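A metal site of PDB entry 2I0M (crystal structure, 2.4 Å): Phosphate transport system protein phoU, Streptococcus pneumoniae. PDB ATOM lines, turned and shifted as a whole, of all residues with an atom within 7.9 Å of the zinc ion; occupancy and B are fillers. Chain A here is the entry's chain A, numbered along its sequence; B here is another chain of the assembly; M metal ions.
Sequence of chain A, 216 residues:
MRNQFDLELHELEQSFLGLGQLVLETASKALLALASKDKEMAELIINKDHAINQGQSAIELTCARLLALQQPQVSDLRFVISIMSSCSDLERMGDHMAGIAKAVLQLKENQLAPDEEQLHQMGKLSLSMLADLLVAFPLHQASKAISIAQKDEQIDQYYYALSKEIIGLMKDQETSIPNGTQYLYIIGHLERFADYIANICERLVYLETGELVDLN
The nearest printed residue that does not touch the zinc ion is Ile 155 (4.8 Å).
The zinc ion is bound by the side-chain carboxylate (OE2) of Glu 191 (2.0 Å), the side-chain carboxylate (OD2) of Asp 156 (2.2 Å) and the side-chain carboxylate (OD1) of Asp 195 (2.5 Å). Slightly farther from the zinc ion lies the side-chain carboxylate (OD2) of Asp 152 (2.7 Å).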
ATOM      1  N   MET A 129       1.914  -6.928  17.599  1.00  0.00           N
ATOM      2  CA  MET A 129       0.566  -6.604  18.055  1.00  0.00           C
ATOM      3  C   MET A 129       0.050  -5.330  17.397  1.00  0.00           C
ATOM      4  O   MET A 129      -1.080  -5.304  16.912  1.00  0.00           O
ATOM      5  CB  MET A 129       0.512  -6.479  19.582  1.00  0.00           C
ATOM      6  CG  MET A 129       0.305  -7.799  20.383  1.00  0.00           C
ATOM      7  SD  MET A 129       0.536  -7.569  22.197  1.00  0.00           S
ATOM      8  CE  MET A 129      -0.996  -6.759  22.602  1.00  0.00           C
ATOM      9  N   ALA A 149      -5.746  -8.602  21.213  1.00  0.00           N
ATOM     10  CA  ALA A 149      -5.837  -8.244  22.639  1.00  0.00           C
ATOM     11  C   ALA A 149      -5.342  -9.365  23.538  1.00  0.00           C
ATOM     12  O   ALA A 149      -4.691  -9.099  24.540  1.00  0.00           O
ATOM     13  CB  ALA A 149      -7.271  -7.852  23.024  1.00  0.00           C
ATOM     14  N   LYS A 151      -3.007 -11.590  23.135  1.00  0.00           N
ATOM     15  CA  LYS A 151      -1.545 -11.680  23.220  1.00  0.00           C
ATOM     16  C   LYS A 151      -0.919 -10.824  24.334  1.00  0.00           C
ATOM     17  O   LYS A 151       0.240 -10.997  24.664  1.00  0.00           O
ATOM     18  CB  LYS A 151      -0.896 -11.346  21.871  1.00  0.00           C
ATOM     19  CG  LYS A 151      -1.193 -12.370  20.806  1.00  0.00           C
ATOM     20  CD  LYS A 151      -0.614 -11.943  19.466  1.00  0.00           C
ATOM     21  CE  LYS A 151      -0.859 -13.008  18.409  1.00  0.00           C
ATOM     22  NZ  LYS A 151       0.140 -12.887  17.316  1.00  0.00           N
ATOM     23  N   ASP A 152      -1.714  -9.918  24.897  1.00  0.00           N
ATOM     24  CA  ASP A 152      -1.283  -9.114  26.049  1.00  0.00           C
ATOM     25  C   ASP A 152      -1.012  -9.950  27.303  1.00  0.00           C
ATOM     26  O   ASP A 152      -0.157  -9.587  28.099  1.00  0.00           O
ATOM     27  CB  ASP A 152      -2.299  -8.007  26.356  1.00  0.00           C
ATOM     28  CG  ASP A 152      -1.747  -6.939  27.287  1.00  0.00           C
ATOM     29  OD1 ASP A 152      -0.672  -6.367  27.001  1.00  0.00           O
ATOM     30  OD2 ASP A 152      -2.393  -6.675  28.304  1.00  0.00           O
ATOM     31  N   GLU A 153      -1.746 -11.067  27.470  1.00  0.00           N
ATOM     32  CA  GLU A 153      -1.427 -12.051  28.508  1.00  0.00           C
ATOM     33  C   GLU A 153       0.070 -12.383  28.505  1.00  0.00           C
ATOM     34  O   GLU A 153       0.712 -12.339  29.544  1.00  0.00           O
ATOM     35  CB  GLU A 153      -2.255 -13.357  28.354  1.00  0.00           C
ATOM     36  CG  GLU A 153      -2.418 -14.159  29.666  1.00  0.00           C
ATOM     37  CD  GLU A 153      -3.010 -15.586  29.480  1.00  0.00           C
ATOM     38  OE1 GLU A 153      -3.531 -15.914  28.391  1.00  0.00           O
ATOM     39  OE2 GLU A 153      -2.949 -16.381  30.440  1.00  0.00           O
ATOM     40  N   GLN A 154       0.618 -12.657  27.321  1.00  0.00           N
ATOM     41  CA  GLN A 154       2.047 -12.972  27.179  1.00  0.00           C
ATOM     42  C   GLN A 154       2.983 -11.817  27.570  1.00  0.00           C
ATOM     43  O   GLN A 154       4.019 -12.051  28.207  1.00  0.00           O
ATOM     44  CB  GLN A 154       2.370 -13.461  25.771  1.00  0.00           C
ATOM     45  CG  GLN A 154       1.981 -14.893  25.502  1.00  0.00           C
ATOM     46  CD  GLN A 154       0.637 -15.027  24.813  1.00  0.00           C
ATOM     47  OE1 GLN A 154      -0.372 -15.351  25.454  1.00  0.00           O
ATOM     48  NE2 GLN A 154       0.615 -14.792  23.498  1.00  0.00           N
ATOM     49  N   ILE A 155       2.620 -10.603  27.183  1.00  0.00           N
ATOM     50  CA  ILE A 155       3.384  -9.415  27.555  1.00  0.00           C
ATOM     51  C   ILE A 155       3.419  -9.194  29.066  1.00  0.00           C
ATOM     52  O   ILE A 155       4.463  -8.849  29.621  1.00  0.00           O
ATOM     53  CB  ILE A 155       2.985  -8.180  26.721  1.00  0.00           C
ATOM     54  CG1 ILE A 155       3.807  -8.184  25.430  1.00  0.00           C
ATOM     55  CG2 ILE A 155       3.240  -6.878  27.462  1.00  0.00           C
ATOM     56  CD1 ILE A 155       3.163  -7.566  24.307  1.00  0.00           C
ATOM     57  N   ASP A 156       2.282  -9.430  29.725  1.00  0.00           N
ATOM     58  CA  ASP A 156       2.193  -9.430  31.175  1.00  0.00           C
ATOM     59  C   ASP A 156       3.141 -10.457  31.806  1.00  0.00           C
ATOM     60  O   ASP A 156       3.814 -10.157  32.795  1.00  0.00           O
ATOM     61  CB  ASP A 156       0.748  -9.676  31.627  1.00  0.00           C
ATOM     62  CG  ASP A 156      -0.129  -8.431  31.462  1.00  0.00           C
ATOM     63  OD1 ASP A 156      -1.371  -8.554  31.625  1.00  0.00           O
ATOM     64  OD2 ASP A 156       0.414  -7.342  31.169  1.00  0.00           O
ATOM     65  N   GLN A 157       3.190 -11.655  31.219  1.00  0.00           N
ATOM     66  CA  GLN A 157       4.100 -12.715  31.665  1.00  0.00           C
ATOM     67  C   GLN A 157       5.564 -12.295  31.500  1.00  0.00           C
ATOM     68  O   GLN A 157       6.374 -12.495  32.400  1.00  0.00           O
ATOM     69  CB  GLN A 157       3.815 -14.006  30.915  1.00  0.00           C
ATOM     70  CG  GLN A 157       2.493 -14.639  31.311  1.00  0.00           C
ATOM     71  CD  GLN A 157       2.036 -15.756  30.366  1.00  0.00           C
ATOM     72  OE1 GLN A 157       0.878 -16.185  30.432  1.00  0.00           O
ATOM     73  NE2 GLN A 157       2.934 -16.244  29.511  1.00  0.00           N
ATOM     74  N   TYR A 159       6.402  -9.194  31.495  1.00  0.00           N
ATOM     75  CA  TYR A 159       6.516  -8.114  32.467  1.00  0.00           C
ATOM     76  C   TYR A 159       6.911  -8.617  33.868  1.00  0.00           C
ATOM     77  O   TYR A 159       7.831  -8.074  34.483  1.00  0.00           O
ATOM     78  CB  TYR A 159       5.234  -7.265  32.521  1.00  0.00           C
ATOM     79  CG  TYR A 159       5.308  -6.156  33.531  1.00  0.00           C
ATOM     80  CD1 TYR A 159       6.165  -5.084  33.339  1.00  0.00           C
ATOM     81  CD2 TYR A 159       4.539  -6.190  34.686  1.00  0.00           C
ATOM     82  CE1 TYR A 159       6.277  -4.066  34.274  1.00  0.00           C
ATOM     83  CE2 TYR A 159       4.636  -5.160  35.632  1.00  0.00           C
ATOM     84  CZ  TYR A 159       5.510  -4.102  35.407  1.00  0.00           C
ATOM     85  OH  TYR A 159       5.613  -3.077  36.322  1.00  0.00           O
ATOM     86  N   TYR A 160       6.229  -9.639  34.372  1.00  0.00           N
ATOM     87  CA  TYR A 160       6.486 -10.122  35.718  1.00  0.00           C
ATOM     88  C   TYR A 160       7.792 -10.903  35.829  1.00  0.00           C
ATOM     89  O   TYR A 160       8.570 -10.658  36.751  1.00  0.00           O
ATOM     90  CB  TYR A 160       5.280 -10.887  36.288  1.00  0.00           C
ATOM     91  CG  TYR A 160       4.078  -9.977  36.539  1.00  0.00           C
ATOM     92  CD1 TYR A 160       4.067  -9.068  37.609  1.00  0.00           C
ATOM     93  CD2 TYR A 160       2.980  -9.997  35.683  1.00  0.00           C
ATOM     94  CE1 TYR A 160       2.975  -8.229  37.827  1.00  0.00           C
ATOM     95  CE2 TYR A 160       1.879  -9.152  35.882  1.00  0.00           C
ATOM     96  CZ  TYR A 160       1.890  -8.272  36.951  1.00  0.00           C
ATOM     97  OH  TYR A 160       0.806  -7.441  37.152  1.00  0.00           O
ATOM     98  N   LEU A 190       6.736  -0.806  27.875  1.00  0.00           N
ATOM     99  CA  LEU A 190       6.293  -1.807  26.915  1.00  0.00           C
ATOM    100  C   LEU A 190       4.984  -2.427  27.361  1.00  0.00           C
ATOM    101  O   LEU A 190       4.100  -2.665  26.536  1.00  0.00           O
ATOM    102  CB  LEU A 190       7.349  -2.922  26.752  1.00  0.00           C
ATOM    103  CG  LEU A 190       8.500  -2.693  25.780  1.00  0.00           C
ATOM    104  CD1 LEU A 190       9.518  -3.819  25.853  1.00  0.00           C
ATOM    105  CD2 LEU A 190       7.950  -2.538  24.363  1.00  0.00           C
ATOM    106  N   GLU A 191       4.873  -2.698  28.656  1.00  0.00           N
ATOM    107  CA  GLU A 191       3.667  -3.286  29.191  1.00  0.00           C
ATOM    108  C   GLU A 191       2.474  -2.325  28.972  1.00  0.00           C
ATOM    109  O   GLU A 191       1.409  -2.783  28.535  1.00  0.00           O
ATOM    110  CB  GLU A 191       3.856  -3.679  30.668  1.00  0.00           C
ATOM    111  CG  GLU A 191       2.778  -4.608  31.239  1.00  0.00           C
ATOM    112  CD  GLU A 191       1.451  -3.904  31.519  1.00  0.00           C
ATOM    113  OE1 GLU A 191       1.464  -2.687  31.831  1.00  0.00           O
ATOM    114  OE2 GLU A 191       0.390  -4.559  31.438  1.00  0.00           O
ATOM    115  N   ARG A 192       2.653  -1.022  29.241  1.00  0.00           N
ATOM    116  CA  ARG A 192       1.640   0.014  28.968  1.00  0.00           C
ATOM    117  C   ARG A 192       1.303   0.181  27.490  1.00  0.00           C
ATOM    118  O   ARG A 192       0.124   0.243  27.134  1.00  0.00           O
ATOM    119  CB  ARG A 192       2.066   1.388  29.518  1.00  0.00           C
ATOM    120  CG  ARG A 192       2.276   1.460  30.989  1.00  0.00           C
ATOM    121  CD  ARG A 192       0.969   1.317  31.737  1.00  0.00           C
ATOM    122  NE  ARG A 192       0.275   2.594  31.858  1.00  0.00           N
ATOM    123  CZ  ARG A 192      -0.644   3.029  30.998  1.00  0.00           C
ATOM    124  NH1 ARG A 192      -0.991   2.273  29.955  1.00  0.00           N
ATOM    125  NH2 ARG A 192      -1.226   4.193  31.187  1.00  0.00           N
ATOM    126  N   PHE A 193       2.330   0.277  26.650  1.00  0.00           N
ATOM    127  CA  PHE A 193       2.199   0.257  25.188  1.00  0.00           C
ATOM    128  C   PHE A 193       1.216  -0.809  24.736  1.00  0.00           C
ATOM    129  O   PHE A 193       0.276  -0.536  24.003  1.00  0.00           O
ATOM    130  CB  PHE A 193       3.576   0.002  24.563  1.00  0.00           C
ATOM    131  CG  PHE A 193       3.614   0.104  23.070  1.00  0.00           C
ATOM    132  CD1 PHE A 193       3.761   1.329  22.431  1.00  0.00           C
ATOM    133  CD2 PHE A 193       3.587  -1.046  22.292  1.00  0.00           C
ATOM    134  CE1 PHE A 193       3.849   1.404  21.034  1.00  0.00           C
ATOM    135  CE2 PHE A 193       3.669  -0.979  20.895  1.00  0.00           C
ATOM    136  CZ  PHE A 193       3.800   0.258  20.267  1.00  0.00           C
ATOM    137  N   ALA A 194       1.444  -2.034  25.201  1.00  0.00           N
ATOM    138  CA  ALA A 194       0.632  -3.184  24.813  1.00  0.00           C
ATOM    139  C   ALA A 194      -0.779  -3.142  25.385  1.00  0.00           C
ATOM    140  O   ALA A 194      -1.735  -3.568  24.741  1.00  0.00           O
ATOM    141  CB  ALA A 194       1.341  -4.491  25.191  1.00  0.00           C
ATOM    142  N   ASP A 195      -0.921  -2.614  26.597  1.00  0.00           N
ATOM    143  CA  ASP A 195      -2.228  -2.387  27.185  1.00  0.00           C
ATOM    144  C   ASP A 195      -3.086  -1.441  26.334  1.00  0.00           C
ATOM    145  O   ASP A 195      -4.262  -1.724  26.104  1.00  0.00           O
ATOM    146  CB  ASP A 195      -2.063  -1.822  28.592  1.00  0.00           C
ATOM    147  CG  ASP A 195      -1.996  -2.903  29.657  1.00  0.00           C
ATOM    148  OD1 ASP A 195      -2.382  -4.057  29.375  1.00  0.00           O
ATOM    149  OD2 ASP A 195      -1.560  -2.585  30.801  1.00  0.00           O
ATOM    150  N   TYR A 196      -2.520  -0.316  25.884  1.00  0.00           N
ATOM    151  CA  TYR A 196      -3.265   0.581  24.979  1.00  0.00           C
ATOM    152  C   TYR A 196      -3.711  -0.069  23.662  1.00  0.00           C
ATOM    153  O   TYR A 196      -4.819   0.206  23.186  1.00  0.00           O
ATOM    154  CB  TYR A 196      -2.502   1.880  24.695  1.00  0.00           C
ATOM    155  CG  TYR A 196      -2.459   2.822  25.876  1.00  0.00           C
ATOM    156  CD1 TYR A 196      -3.625   3.383  26.393  1.00  0.00           C
ATOM    157  CD2 TYR A 196      -1.246   3.135  26.508  1.00  0.00           C
ATOM    158  CE1 TYR A 196      -3.601   4.252  27.509  1.00  0.00           C
ATOM    159  CE2 TYR A 196      -1.217   3.987  27.621  1.00  0.00           C
ATOM    160  CZ  TYR A 196      -2.389   4.542  28.102  1.00  0.00           C
ATOM    161  OH  TYR A 196      -2.353   5.389  29.185  1.00  0.00           O
ATOM    162  N   ALA A 198      -4.543  -3.160  23.378  1.00  0.00           N
ATOM    163  CA  ALA A 198      -5.678  -3.954  23.817  1.00  0.00           C
ATOM    164  C   ALA A 198      -6.927  -3.081  23.963  1.00  0.00           C
ATOM    165  O   ALA A 198      -8.015  -3.470  23.546  1.00  0.00           O
ATOM    166  CB  ALA A 198      -5.343  -4.663  25.150  1.00  0.00           C
ATOM    167  N   ARG B 192      -1.999   2.241  37.847  1.00  0.00           N
ATOM    168  CA  ARG B 192      -2.749   2.602  36.626  1.00  0.00           C
ATOM    169  C   ARG B 192      -3.879   3.595  36.871  1.00  0.00           C
ATOM    170  O   ARG B 192      -4.014   4.573  36.135  1.00  0.00           O
ATOM    171  CB  ARG B 192      -3.350   1.366  35.941  1.00  0.00           C
ATOM    172  CG  ARG B 192      -2.364   0.347  35.463  1.00  0.00           C
ATOM    173  CD  ARG B 192      -1.546   0.877  34.316  1.00  0.00           C
ATOM    174  NE  ARG B 192      -2.222   0.685  33.031  1.00  0.00           N
ATOM    175  CZ  ARG B 192      -3.011   1.599  32.468  1.00  0.00           C
ATOM    176  NH1 ARG B 192      -3.200   2.781  33.060  1.00  0.00           N
ATOM    177  NH2 ARG B 192      -3.576   1.345  31.303  1.00  0.00           N
HETATM  178 ZN    ZN M   1      -0.612  -5.690  30.128  1.00  0.00          ZN
